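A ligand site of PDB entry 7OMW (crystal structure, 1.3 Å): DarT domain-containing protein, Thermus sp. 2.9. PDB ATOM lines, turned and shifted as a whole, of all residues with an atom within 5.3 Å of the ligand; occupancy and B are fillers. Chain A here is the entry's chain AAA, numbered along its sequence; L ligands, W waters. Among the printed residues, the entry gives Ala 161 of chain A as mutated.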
ATOM      1  N   TYR A  13      27.430   1.473 -13.452  1.00  0.00           N
ATOM      2  CA  TYR A  13      25.988   1.669 -13.574  1.00  0.00           C
ATOM      3  C   TYR A  13      25.634   2.037 -15.008  1.00  0.00           C
ATOM      4  O   TYR A  13      26.234   2.970 -15.592  1.00  0.00           O
ATOM      5  CB  TYR A  13      25.553   2.836 -12.665  1.00  0.00           C
ATOM      6  CG  TYR A  13      25.946   2.642 -11.214  1.00  0.00           C
ATOM      7  CD1 TYR A  13      27.191   2.989 -10.758  1.00  0.00           C
ATOM      8  CD2 TYR A  13      25.062   2.144 -10.293  1.00  0.00           C
ATOM      9  CE1 TYR A  13      27.576   2.854  -9.445  1.00  0.00           C
ATOM     10  CE2 TYR A  13      25.431   1.946  -8.983  1.00  0.00           C
ATOM     11  CZ  TYR A  13      26.687   2.299  -8.534  1.00  0.00           C
ATOM     12  OH  TYR A  13      27.018   2.147  -7.205  1.00  0.00           O
ATOM     13  N   HIS A  14      24.645   1.363 -15.573  1.00  0.00           N
ATOM     14  CA  HIS A  14      24.063   1.727 -16.893  1.00  0.00           C
ATOM     15  C   HIS A  14      22.621   1.983 -16.653  1.00  0.00           C
ATOM     16  O   HIS A  14      21.864   1.137 -16.216  1.00  0.00           O
ATOM     17  CB  HIS A  14      24.240   0.573 -17.912  1.00  0.00           C
ATOM     18  CG  HIS A  14      23.600   0.841 -19.231  1.00  0.00           C
ATOM     19  ND1 HIS A  14      24.255   1.522 -20.248  1.00  0.00           N
ATOM     20  CD2 HIS A  14      22.368   0.511 -19.681  1.00  0.00           C
ATOM     21  CE1 HIS A  14      23.422   1.604 -21.288  1.00  0.00           C
ATOM     22  NE2 HIS A  14      22.256   1.002 -21.008  1.00  0.00           N
ATOM     23  N   ILE A  15      22.158   3.200 -17.009  1.00  0.00           N
ATOM     24  CA  ILE A  15      20.719   3.554 -16.897  1.00  0.00           C
ATOM     25  C   ILE A  15      20.033   3.288 -18.219  1.00  0.00           C
ATOM     26  O   ILE A  15      20.592   3.568 -19.282  1.00  0.00           O
ATOM     27  CB  ILE A  15      20.475   4.977 -16.370  1.00  0.00           C
ATOM     28  CG1 ILE A  15      21.154   6.082 -17.178  1.00  0.00           C
ATOM     29  CG2 ILE A  15      20.846   5.039 -14.904  1.00  0.00           C
ATOM     30  CD1 ILE A  15      20.645   7.475 -16.830  1.00  0.00           C
ATOM     31  N   THR A  16      18.821   2.763 -18.136  1.00  0.00           N
ATOM     32  CA  THR A  16      18.028   2.484 -19.349  1.00  0.00           C
ATOM     33  C   THR A  16      16.563   2.455 -18.973  1.00  0.00           C
ATOM     34  O   THR A  16      16.193   2.118 -17.845  1.00  0.00           O
ATOM     35  CB  THR A  16      18.461   1.170 -20.024  1.00  0.00           C
ATOM     36  OG1 THR A  16      17.925   1.178 -21.360  1.00  0.00           O
ATOM     37  CG2 THR A  16      18.017  -0.072 -19.288  1.00  0.00           C
ATOM     38  N   ASN A  20      13.191  -1.131 -22.425  1.00  0.00           N
ATOM     39  CA  ASN A  20      14.342  -1.785 -23.087  1.00  0.00           C
ATOM     40  C   ASN A  20      14.724  -3.114 -22.404  1.00  0.00           C
ATOM     41  O   ASN A  20      15.491  -3.847 -23.001  1.00  0.00           O
ATOM     42  CB  ASN A  20      15.569  -0.888 -23.118  1.00  0.00           C
ATOM     43  CG  ASN A  20      15.275   0.398 -23.870  1.00  0.00           C
ATOM     44  OD1 ASN A  20      14.490   0.409 -24.807  1.00  0.00           O
ATOM     45  ND2 ASN A  20      15.921   1.470 -23.466  1.00  0.00           N
ATOM     46  N   GLY A  23      14.207  -6.448 -24.371  1.00  0.00           N
ATOM     47  CA  GLY A  23      15.161  -6.663 -25.475  1.00  0.00           C
ATOM     48  C   GLY A  23      16.537  -7.078 -24.988  1.00  0.00           C
ATOM     49  O   GLY A  23      17.232  -7.840 -25.679  1.00  0.00           O
ATOM     50  N   ILE A  24      16.909  -6.577 -23.824  1.00  0.00           N
ATOM     51  CA  ILE A  24      18.208  -6.957 -23.214  1.00  0.00           C
ATOM     52  C   ILE A  24      18.167  -8.446 -22.779  1.00  0.00           C
ATOM     53  O   ILE A  24      19.086  -9.209 -23.076  1.00  0.00           O
ATOM     54  CB  ILE A  24      18.540  -6.032 -22.043  1.00  0.00           C
ATOM     55  CG1 ILE A  24      18.740  -4.585 -22.563  1.00  0.00           C
ATOM     56  CG2 ILE A  24      19.737  -6.547 -21.270  1.00  0.00           C
ATOM     57  CD1 ILE A  24      18.717  -3.515 -21.502  1.00  0.00           C
ATOM     58  N   MET A  27      18.084 -10.822 -25.872  1.00  0.00           N
ATOM     59  CA  MET A  27      19.399 -10.849 -26.572  1.00  0.00           C
ATOM     60  C   MET A  27      20.400 -11.557 -25.647  1.00  0.00           C
ATOM     61  O   MET A  27      21.409 -12.076 -26.164  1.00  0.00           O
ATOM     62  CB  MET A  27      19.857  -9.399 -26.887  1.00  0.00           C
ATOM     63  CG  MET A  27      20.994  -9.199 -27.840  1.00  0.00           C
ATOM     64  SD  MET A  27      20.690  -9.866 -29.461  1.00  0.00           S
ATOM     65  CE  MET A  27      19.669  -8.589 -30.185  1.00  0.00           C
ATOM     66  N   LYS A  29      22.177  -9.683 -23.648  1.00  0.00           N
ATOM     67  CA  LYS A  29      23.284  -8.716 -23.581  1.00  0.00           C
ATOM     68  C   LYS A  29      22.762  -7.317 -23.910  1.00  0.00           C
ATOM     69  O   LYS A  29      21.779  -7.201 -24.626  1.00  0.00           O
ATOM     70  CB  LYS A  29      24.427  -9.129 -24.476  1.00  0.00           C
ATOM     71  CG  LYS A  29      24.035  -9.447 -25.895  1.00  0.00           C
ATOM     72  CD  LYS A  29      25.091 -10.072 -26.740  1.00  0.00           C
ATOM     73  CE  LYS A  29      24.561 -10.698 -28.023  1.00  0.00           C
ATOM     74  NZ  LYS A  29      25.617 -11.451 -28.744  1.00  0.00           N
ATOM     75  N   LEU A  30      23.483  -6.361 -23.351  1.00  0.00           N
ATOM     76  CA  LEU A  30      23.422  -4.952 -23.854  1.00  0.00           C
ATOM     77  C   LEU A  30      24.292  -4.912 -25.113  1.00  0.00           C
ATOM     78  O   LEU A  30      25.395  -5.456 -25.114  1.00  0.00           O
ATOM     79  CB  LEU A  30      23.972  -3.971 -22.811  1.00  0.00           C
ATOM     80  CG  LEU A  30      23.142  -3.737 -21.541  1.00  0.00           C
ATOM     81  CD1 LEU A  30      23.964  -3.140 -20.383  1.00  0.00           C
ATOM     82  CD2 LEU A  30      21.996  -2.787 -21.837  1.00  0.00           C
ATOM     83  N   LEU A  31      23.821  -4.199 -26.133  1.00  0.00           N
ATOM     84  CA  LEU A  31      24.606  -3.967 -27.370  1.00  0.00           C
ATOM     85  C   LEU A  31      24.980  -2.491 -27.451  1.00  0.00           C
ATOM     86  O   LEU A  31      24.151  -1.607 -27.145  1.00  0.00           O
ATOM     87  CB  LEU A  31      23.779  -4.395 -28.585  1.00  0.00           C
ATOM     88  CG  LEU A  31      23.497  -5.883 -28.713  1.00  0.00           C
ATOM     89  CD1 LEU A  31      22.575  -6.160 -29.884  1.00  0.00           C
ATOM     90  CD2 LEU A  31      24.778  -6.690 -28.851  1.00  0.00           C
ATOM     91  N   HIS A  33      25.675   1.088 -29.299  1.00  0.00           N
ATOM     92  CA  HIS A  33      24.931   1.838 -30.345  1.00  0.00           C
ATOM     93  C   HIS A  33      25.240   1.257 -31.739  1.00  0.00           C
ATOM     94  O   HIS A  33      24.312   1.014 -32.531  1.00  0.00           O
ATOM     95  CB  HIS A  33      25.301   3.300 -30.200  1.00  0.00           C
ATOM     96  CG  HIS A  33      24.634   4.173 -31.199  1.00  0.00           C
ATOM     97  ND1 HIS A  33      25.030   4.310 -32.519  1.00  0.00           N
ATOM     98  CD2 HIS A  33      23.534   4.922 -31.039  1.00  0.00           C
ATOM     99  CE1 HIS A  33      24.231   5.166 -33.135  1.00  0.00           C
ATOM    100  NE2 HIS A  33      23.289   5.520 -32.245  1.00  0.00           N
ATOM    101  N   PRO A  37      21.278  -2.078 -31.089  1.00  0.00           N
ATOM    102  CA  PRO A  37      20.430  -2.598 -30.028  1.00  0.00           C
ATOM    103  C   PRO A  37      18.978  -2.416 -30.394  1.00  0.00           C
ATOM    104  O   PRO A  37      18.596  -1.352 -30.891  1.00  0.00           O
ATOM    105  CB  PRO A  37      20.829  -1.776 -28.806  1.00  0.00           C
ATOM    106  CG  PRO A  37      21.353  -0.470 -29.378  1.00  0.00           C
ATOM    107  CD  PRO A  37      22.069  -0.904 -30.645  1.00  0.00           C
ATOM    108  N   PRO A  38      18.112  -3.406 -30.129  1.00  0.00           N
ATOM    109  CA  PRO A  38      16.664  -3.295 -30.360  1.00  0.00           C
ATOM    110  C   PRO A  38      15.977  -2.471 -29.263  1.00  0.00           C
ATOM    111  O   PRO A  38      15.036  -2.916 -28.615  1.00  0.00           O
ATOM    112  CB  PRO A  38      16.194  -4.744 -30.422  1.00  0.00           C
ATOM    113  CG  PRO A  38      17.138  -5.437 -29.445  1.00  0.00           C
ATOM    114  CD  PRO A  38      18.479  -4.763 -29.693  1.00  0.00           C
ATOM    115  N   LYS A  39      16.479  -1.259 -29.055  1.00  0.00           N
ATOM    116  CA  LYS A  39      15.920  -0.369 -28.032  1.00  0.00           C
ATOM    117  C   LYS A  39      14.514   0.082 -28.437  1.00  0.00           C
ATOM    118  O   LYS A  39      14.210   0.217 -29.638  1.00  0.00           O
ATOM    119  CB  LYS A  39      16.848   0.828 -27.844  1.00  0.00           C
ATOM    120  CG  LYS A  39      16.911   1.818 -29.009  1.00  0.00           C
ATOM    121  CD  LYS A  39      18.094   2.757 -28.960  1.00  0.00           C
ATOM    122  CE  LYS A  39      18.087   3.714 -30.146  1.00  0.00           C
ATOM    123  NZ  LYS A  39      19.132   4.739 -30.042  1.00  0.00           N
ATOM    124  N   GLN A  40      13.685   0.262 -27.425  1.00  0.00           N
ATOM    125  CA  GLN A  40      12.304   0.781 -27.605  1.00  0.00           C
ATOM    126  C   GLN A  40      12.247   2.248 -27.236  1.00  0.00           C
ATOM    127  O   GLN A  40      11.335   2.908 -27.702  1.00  0.00           O
ATOM    128  CB  GLN A  40      11.337   0.001 -26.728  1.00  0.00           C
ATOM    129  CG  GLN A  40      11.197  -1.447 -27.160  1.00  0.00           C
ATOM    130  CD  GLN A  40      10.834  -1.583 -28.616  1.00  0.00           C
ATOM    131  OE1 GLN A  40       9.869  -0.994 -29.063  1.00  0.00           O
ATOM    132  NE2 GLN A  40      11.586  -2.394 -29.343  1.00  0.00           N
ATOM    133  N   ARG A  41      13.129   2.732 -26.363  1.00  0.00           N
ATOM    134  CA  ARG A  41      13.101   4.130 -25.905  1.00  0.00           C
ATOM    135  C   ARG A  41      14.508   4.637 -25.739  1.00  0.00           C
ATOM    136  O   ARG A  41      15.311   4.023 -25.020  1.00  0.00           O
ATOM    137  CB  ARG A  41      12.510   4.363 -24.517  1.00  0.00           C
ATOM    138  CG  ARG A  41      11.124   3.816 -24.352  1.00  0.00           C
ATOM    139  CD  ARG A  41      10.156   4.925 -24.540  1.00  0.00           C
ATOM    140  NE  ARG A  41       8.969   4.482 -23.876  1.00  0.00           N
ATOM    141  CZ  ARG A  41       7.881   5.195 -23.772  1.00  0.00           C
ATOM    142  NH1 ARG A  41       6.838   4.691 -23.147  1.00  0.00           N
ATOM    143  NH2 ARG A  41       7.835   6.402 -24.314  1.00  0.00           N
ATOM    144  N   SER A  42      14.790   5.701 -26.458  1.00  0.00           N
ATOM    145  CA  SER A  42      16.019   6.500 -26.306  1.00  0.00           C
ATOM    146  C   SER A  42      15.816   7.525 -25.190  1.00  0.00           C
ATOM    147  O   SER A  42      14.756   8.165 -25.142  1.00  0.00           O
ATOM    148  CB  SER A  42      16.321   7.223 -27.584  1.00  0.00           C
ATOM    149  OG  SER A  42      17.406   8.107 -27.390  1.00  0.00           O
ATOM    150  N   ILE A  43      16.776   7.622 -24.279  1.00  0.00           N
ATOM    151  CA  ILE A  43      16.826   8.603 -23.174  1.00  0.00           C
ATOM    152  C   ILE A  43      18.149   9.409 -23.342  1.00  0.00           C
ATOM    153  O   ILE A  43      18.230  10.207 -22.281  1.00  0.00           O
ATOM    154  CB  ILE A  43      16.682   7.928 -21.779  1.00  0.00           C
ATOM    155  CG1 ILE A  43      17.883   7.057 -21.406  1.00  0.00           C
ATOM    156  CG2 ILE A  43      15.379   7.158 -21.693  1.00  0.00           C
ATOM    157  CD1 ILE A  43      17.881   6.440 -20.000  1.00  0.00           C
ATOM    158  N   ARG A  52      29.014  11.147 -30.520  1.00  0.00           N
ATOM    159  CA  ARG A  52      29.693   9.886 -30.091  1.00  0.00           C
ATOM    160  C   ARG A  52      30.086   8.991 -31.277  1.00  0.00           C
ATOM    161  O   ARG A  52      30.794   7.945 -31.087  1.00  0.00           O
ATOM    162  CB  ARG A  52      28.776   9.105 -29.150  1.00  0.00           C
ATOM    163  CG  ARG A  52      28.699   9.641 -27.731  1.00  0.00           C
ATOM    164  CD  ARG A  52      27.756  10.801 -27.593  1.00  0.00           C
ATOM    165  NE  ARG A  52      27.471  11.081 -26.190  1.00  0.00           N
ATOM    166  CZ  ARG A  52      27.087  12.250 -25.715  1.00  0.00           C
ATOM    167  NH1 ARG A  52      26.928  13.272 -26.542  1.00  0.00           N
ATOM    168  NH2 ARG A  52      26.863  12.399 -24.423  1.00  0.00           N
ATOM    169  N   HIS A  66      30.562   5.134 -29.642  1.00  0.00           N
ATOM    170  CA  HIS A  66      29.355   4.356 -30.014  1.00  0.00           C
ATOM    171  C   HIS A  66      29.658   2.869 -30.257  1.00  0.00           C
ATOM    172  O   HIS A  66      28.705   2.117 -30.483  1.00  0.00           O
ATOM    173  CB  HIS A  66      28.659   4.991 -31.223  1.00  0.00           C
ATOM    174  CG  HIS A  66      27.676   6.055 -30.882  1.00  0.00           C
ATOM    175  ND1 HIS A  66      27.103   6.872 -31.837  1.00  0.00           N
ATOM    176  CD2 HIS A  66      27.106   6.387 -29.713  1.00  0.00           C
ATOM    177  CE1 HIS A  66      26.212   7.656 -31.250  1.00  0.00           C
ATOM    178  NE2 HIS A  66      26.193   7.370 -29.960  1.00  0.00           N
ATOM    179  N   TYR A  68      30.943   1.114 -27.899  1.00  0.00           N
ATOM    180  CA  TYR A  68      31.005   0.574 -26.519  1.00  0.00           C
ATOM    181  C   TYR A  68      29.663   0.711 -25.828  1.00  0.00           C
ATOM    182  O   TYR A  68      28.929   1.681 -26.078  1.00  0.00           O
ATOM    183  CB  TYR A  68      32.068   1.303 -25.679  1.00  0.00           C
ATOM    184  CG  TYR A  68      33.472   1.199 -26.215  1.00  0.00           C
ATOM    185  CD1 TYR A  68      33.895   1.883 -27.337  1.00  0.00           C
ATOM    186  CD2 TYR A  68      34.417   0.401 -25.567  1.00  0.00           C
ATOM    187  CE1 TYR A  68      35.177   1.774 -27.840  1.00  0.00           C
ATOM    188  CE2 TYR A  68      35.712   0.306 -26.022  1.00  0.00           C
ATOM    189  CZ  TYR A  68      36.082   0.924 -27.209  1.00  0.00           C
ATOM    190  OH  TYR A  68      37.375   0.782 -27.621  1.00  0.00           O
ATOM    191  N   VAL A  69      29.368  -0.213 -24.902  1.00  0.00           N
ATOM    192  CA  VAL A  69      28.261  -0.064 -23.948  1.00  0.00           C
ATOM    193  C   VAL A  69      28.763   0.812 -22.808  1.00  0.00           C
ATOM    194  O   VAL A  69      29.778   0.516 -22.187  1.00  0.00           O
ATOM    195  CB  VAL A  69      27.818  -1.430 -23.398  1.00  0.00           C
ATOM    196  CG1 VAL A  69      26.703  -1.231 -22.417  1.00  0.00           C
ATOM    197  CG2 VAL A  69      27.454  -2.338 -24.563  1.00  0.00           C
ATOM    198  N   PRO A  70      28.076   1.944 -22.523  1.00  0.00           N
ATOM    199  CA  PRO A  70      28.584   2.887 -21.548  1.00  0.00           C
ATOM    200  C   PRO A  70      28.007   2.747 -20.155  1.00  0.00           C
ATOM    201  O   PRO A  70      26.832   2.493 -20.009  1.00  0.00           O
ATOM    202  CB  PRO A  70      28.113   4.225 -22.177  1.00  0.00           C
ATOM    203  CG  PRO A  70      26.766   3.913 -22.765  1.00  0.00           C
ATOM    204  CD  PRO A  70      26.941   2.501 -23.306  1.00  0.00           C
ATOM    205  N   PHE A  71      28.862   2.946 -19.169  1.00  0.00           N
ATOM    206  CA  PHE A  71      28.501   2.966 -17.753  1.00  0.00           C
ATOM    207  C   PHE A  71      29.120   4.179 -17.103  1.00  0.00           C
ATOM    208  O   PHE A  71      30.168   4.665 -17.532  1.00  0.00           O
ATOM    209  CB  PHE A  71      29.096   1.728 -17.048  1.00  0.00           C
ATOM    210  CG  PHE A  71      28.529   0.384 -17.479  1.00  0.00           C
ATOM    211  CD1 PHE A  71      28.876  -0.188 -18.675  1.00  0.00           C
ATOM    212  CD2 PHE A  71      27.638  -0.300 -16.661  1.00  0.00           C
ATOM    213  CE1 PHE A  71      28.357  -1.410 -19.075  1.00  0.00           C
ATOM    214  CE2 PHE A  71      27.108  -1.528 -17.054  1.00  0.00           C
ATOM    215  CZ  PHE A  71      27.451  -2.057 -18.266  1.00  0.00           C
ATOM    216  N   TYR A  72      28.463   4.653 -16.055  1.00  0.00           N
ATOM    217  CA  TYR A  72      29.083   5.595 -15.106  1.00  0.00           C
ATOM    218  C   TYR A  72      29.566   4.866 -13.878  1.00  0.00           C
ATOM    219  O   TYR A  72      29.204   3.724 -13.678  1.00  0.00           O
ATOM    220  CB  TYR A  72      28.118   6.734 -14.749  1.00  0.00           C
ATOM    221  CG  TYR A  72      27.801   7.693 -15.861  1.00  0.00           C
ATOM    222  CD1 TYR A  72      28.822   8.376 -16.503  1.00  0.00           C
ATOM    223  CD2 TYR A  72      26.497   7.927 -16.267  1.00  0.00           C
ATOM    224  CE1 TYR A  72      28.550   9.275 -17.521  1.00  0.00           C
ATOM    225  CE2 TYR A  72      26.219   8.843 -17.253  1.00  0.00           C
ATOM    226  CZ  TYR A  72      27.248   9.464 -17.903  1.00  0.00           C
ATOM    227  OH  TYR A  72      26.909  10.361 -18.884  1.00  0.00           O
ATOM    228  N   MET A  79      23.091  12.911 -16.159  1.00  0.00           N
ATOM    229  CA  MET A  79      22.169  12.439 -17.215  1.00  0.00           C
ATOM    230  C   MET A  79      20.796  12.200 -16.634  1.00  0.00           C
ATOM    231  O   MET A  79      19.757  12.581 -17.195  1.00  0.00           O
ATOM    232  CB  MET A  79      22.739  11.216 -17.916  1.00  0.00           C
ATOM    233  CG  MET A  79      21.847  10.637 -18.983  1.00  0.00           C
ATOM    234  SD  MET A  79      22.627   9.183 -19.714  1.00  0.00           S
ATOM    235  CE  MET A  79      21.276   8.519 -20.651  1.00  0.00           C
ATOM    236  N   HIS A 120      34.000  13.035 -18.478  1.00  0.00           N
ATOM    237  CA  HIS A 120      33.042  12.906 -19.611  1.00  0.00           C
ATOM    238  C   HIS A 120      33.783  12.507 -20.898  1.00  0.00           C
ATOM    239  O   HIS A 120      34.659  13.253 -21.313  1.00  0.00           O
ATOM    240  CB  HIS A 120      32.349  14.265 -19.696  1.00  0.00           C
ATOM    241  CG  HIS A 120      31.123  14.357 -20.512  1.00  0.00           C
ATOM    242  ND1 HIS A 120      30.491  13.250 -20.982  1.00  0.00           N
ATOM    243  CD2 HIS A 120      30.378  15.427 -20.884  1.00  0.00           C
ATOM    244  CE1 HIS A 120      29.399  13.599 -21.622  1.00  0.00           C
ATOM    245  NE2 HIS A 120      29.308  14.944 -21.592  1.00  0.00           N
ATOM    246  N   VAL A 122      33.228  12.397 -24.055  1.00  0.00           N
ATOM    247  CA  VAL A 122      33.083  13.266 -25.256  1.00  0.00           C
ATOM    248  C   VAL A 122      34.031  14.468 -25.177  1.00  0.00           C
ATOM    249  O   VAL A 122      34.108  15.179 -26.186  1.00  0.00           O
ATOM    250  CB  VAL A 122      31.626  13.738 -25.451  1.00  0.00           C
ATOM    251  CG1 VAL A 122      30.714  12.578 -25.786  1.00  0.00           C
ATOM    252  CG2 VAL A 122      31.102  14.513 -24.252  1.00  0.00           C
ATOM    253  N   ALA A 161      33.602   7.564 -17.283  1.00  0.00           N
ATOM    254  CA  ALA A 161      32.826   6.459 -17.847  1.00  0.00           C
ATOM    255  C   ALA A 161      33.657   5.199 -17.954  1.00  0.00           C
ATOM    256  O   ALA A 161      34.877   5.232 -18.136  1.00  0.00           O
ATOM    257  CB  ALA A 161      32.300   6.863 -19.222  1.00  0.00           C
HETATM  258  P1  LIG L   1      23.784   3.977 -25.785  1.00  0.00           P
HETATM  259  O1  LIG L   1      24.717   4.470 -26.821  1.00  0.00           O
HETATM  260  O2  LIG L   1      24.266   2.812 -24.970  1.00  0.00           O
HETATM  261  O3  LIG L   1      22.328   3.691 -26.394  1.00  0.00           O
HETATM  262  C1  LIG L   1      21.847   2.365 -26.573  1.00  0.00           C
HETATM  263  C2  LIG L   1      20.471   2.202 -25.981  1.00  0.00           C
HETATM  264  O4  LIG L   1      20.015   0.849 -26.273  1.00  0.00           O
HETATM  265  C3  LIG L   1      20.428   2.326 -24.454  1.00  0.00           C
HETATM  266  O5  LIG L   1      19.212   2.857 -23.951  1.00  0.00           O
HETATM  267  C4  LIG L   1      20.611   0.869 -24.014  1.00  0.00           C
HETATM  268  O6  LIG L   1      20.222   0.546 -22.691  1.00  0.00           O
HETATM  269  C5  LIG L   1      19.728   0.191 -25.033  1.00  0.00           C
HETATM  270  N1  LIG L   1      20.002  -1.234 -25.242  1.00  0.00           N
HETATM  271  C6  LIG L   1      21.235  -1.834 -25.316  1.00  0.00           C
HETATM  272  N2  LIG L   1      21.143  -3.110 -25.606  1.00  0.00           N
HETATM  273  C7  LIG L   1      19.788  -3.360 -25.739  1.00  0.00           C
HETATM  274  C8  LIG L   1      19.044  -4.494 -26.062  1.00  0.00           C
HETATM  275  N3  LIG L   1      19.565  -5.723 -26.255  1.00  0.00           N
HETATM  276  N4  LIG L   1      17.696  -4.376 -26.144  1.00  0.00           N
HETATM  277  C9  LIG L   1      17.131  -3.171 -25.923  1.00  0.00           C
HETATM  278  N5  LIG L   1      17.746  -2.054 -25.601  1.00  0.00           N
HETATM  279  C10 LIG L   1      19.062  -2.187 -25.539  1.00  0.00           C
HETATM  280  O7  LIG L   1      23.564   5.212 -24.826  1.00  0.00           O
HETATM  281  P2  LIG L   1      22.439   5.927 -24.002  1.00  0.00           P
HETATM  282  O8  LIG L   1      22.071   5.132 -22.813  1.00  0.00           O
HETATM  283  O9  LIG L   1      21.414   6.442 -24.891  1.00  0.00           O
HETATM  284  O10 LIG L   1      23.351   7.122 -23.496  1.00  0.00           O
HETATM  285  C11 LIG L   1      23.526   8.333 -24.205  1.00  0.00           C
HETATM  286  C12 LIG L   1      24.928   8.823 -23.960  1.00  0.00           C
HETATM  287  O11 LIG L   1      25.093   9.077 -22.562  1.00  0.00           O
HETATM  288  C13 LIG L   1      26.075   7.908 -24.354  1.00  0.00           C
HETATM  289  O12 LIG L   1      26.338   7.984 -25.746  1.00  0.00           O
HETATM  290  C14 LIG L   1      27.194   8.428 -23.453  1.00  0.00           C
HETATM  291  O13 LIG L   1      27.831   9.565 -23.985  1.00  0.00           O
HETATM  292  C15 LIG L   1      26.443   8.777 -22.166  1.00  0.00           C
HETATM  293  N6  LIG L   1      26.435   7.667 -21.184  1.00  0.00           N
HETATM  294  C16 LIG L   1      25.308   6.950 -20.894  1.00  0.00           C
HETATM  295  C17 LIG L   1      25.366   6.003 -19.891  1.00  0.00           C
HETATM  296  C18 LIG L   1      24.164   5.198 -19.446  1.00  0.00           C
HETATM  297  O14 LIG L   1      24.185   4.850 -18.303  1.00  0.00           O
HETATM  298  N7  LIG L   1      23.151   4.959 -20.267  1.00  0.00           N
HETATM  299  C19 LIG L   1      26.562   5.812 -19.160  1.00  0.00           C
HETATM  300  C20 LIG L   1      27.678   6.548 -19.481  1.00  0.00           C
HETATM  301  C21 LIG L   1      27.605   7.443 -20.506  1.00  0.00           C
HETATM  302  O   HOH W   1      19.788   4.299 -21.862  1.00  0.00           O
HETATM  303  O   HOH W   2      20.312   6.160 -27.682  1.00  0.00           O
HETATM  304  O   HOH W   3      26.753   2.687 -27.256  1.00  0.00           O
HETATM  305  O   HOH W   4      18.862   5.531 -24.970  1.00  0.00           O
HETATM  306  O   HOH W   5      24.611   8.565 -27.855  1.00  0.00           O
HETATM  307  O   HOH W   6      26.963   5.761 -26.627  1.00  0.00           O
HETATM  308  O   HOH W   7      16.753   4.228 -22.288  1.00  0.00           O
HETATM  309  O   HOH W   8      19.887   8.347 -26.387  1.00  0.00           O
HETATM  310  O   HOH W   9      24.772   5.225 -15.698  1.00  0.00           O
HETATM  311  O   HOH W  10      24.198   0.128 -24.901  1.00  0.00           O
HETATM  312  O   HOH W  11      21.213   3.388 -29.784  1.00  0.00           O
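SD of Met 79 sits close to O11 of the ligand (3.8 Å). Tyr 13 touches the ligand (O to O14, 3.9 Å). Asn 20 touches the ligand. Met 27 touches the ligand. Leu 30 touches the ligand. His 33 touches the ligand (CB to O1, 3.6 Å). CB of Pro 37 touches N2 of the ligand, 3.5 Å away. O of Pro 38 touches C9 of the ligand (3.4 Å). Lys 39 touches the ligand (CA to N5, 3.5 Å). CD of Pro 70 touches O2 of the ligand (3.2 Å). C of Phe 71 touches C20 of the ligand, at 3.7 Å. Tyr 72 touches the ligand (CZ to C21, 3.3 Å). Of the 30 residues printed, 20 come within 4 Å of the ligand. The nearest printed residue that does not touch the ligand is Arg 41 (4.2 Å).
ND1 of His 14 lies within hydrogen-bond range of O of Pro 70. A ring nitrogen (ND1) of His 33 sits at hydrogen-bond distance from a ring nitrogen (ND1) of His 66, at 3.4 Å. OG1 of Thr 16 is in hydrogen-bond range of ND2 of Asn 20. The backbone NH (N) of Lys 29 sits at hydrogen-bond distance from the backbone carbonyl oxygen (O) of Ile 24 (3.2 Å). N of Gln 40 lies within hydrogen-bond range of OD1 of Asn 20. N of His 66 lies within hydrogen-bond range of O of Arg 52 (3.2 Å). O of Arg 41 sits at hydrogen-bond distance from ND2 of Asn 20, 3.1 Å away. The backbone carbonyl oxygen (O) of Tyr 13 lies within hydrogen-bond range of the backbone NH (N) of Tyr 72, 2.8 Å away.
O13 of the ligand sits at hydrogen-bond distance from NE of Arg 52, 2.7 Å away. An oxygen (O6) of the ligand lies within hydrogen-bond range of a ring nitrogen (NE2) of His 14, at 2.7 Å. The side-chain hydroxyl of Thr 16 sits at hydrogen-bond distance from an oxygen (O6) of the ligand (2.7 Å). O of Lys 29 is in hydrogen-bond range of N3 of the ligand, 3.1 Å away. A nitrogen (N4) of the ligand lies within hydrogen-bond range of the backbone NH (N) of Ile 24 (3.3 Å). O14 of the ligand is in hydrogen-bond range of N of Ile 15 (2.9 Å). A nitrogen (N2) of the ligand sits at hydrogen-bond distance from the backbone NH (N) of Leu 31 (2.9 Å). The backbone carbonyl oxygen (O) of Ile 15 sits at hydrogen-bond distance from a nitrogen (N7) of the ligand (3.1 Å). A nitrogen (N3) of the ligand sits at hydrogen-bond distance from the backbone carbonyl oxygen (O) of Gly 23 (3.2 Å).
Water W1 lies within hydrogen-bond range of an oxygen (O5) of the ligand (2.6 Å) and the backbone carbonyl oxygen of Ile 15 (2.8 Å). Water W10 lies within hydrogen-bond range of an oxygen (O2) of the ligand (2.7 Å) and the backbone carbonyl oxygen (O) of Leu 31 (2.8 Å). Water W9 bridges the backbone carbonyl oxygen of Tyr 13 (2.7 Å) and an oxygen (O14) of the ligand (2.7 Å). Water W3 lies within hydrogen-bond range of the backbone carbonyl oxygen (O) of Tyr 68 (2.7 Å), an oxygen (O1) of the ligand (2.7 Å) and the backbone NH (N) of His 33 (2.8 Å). Water W5 bridges an oxygen (O12) of the ligand (2.8 Å) and a ring nitrogen (NE2) of His 66 (2.9 Å). Water W7 lies within hydrogen-bond range of the backbone carbonyl oxygen (O) of Arg 41 (3.1 Å), the side-chain amide nitrogen (ND2) of Asn 20 (3.1 Å), an oxygen (O5) of the ligand (3.3 Å) and the side-chain hydroxyl (OG1) of Thr 16 (3.4 Å).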
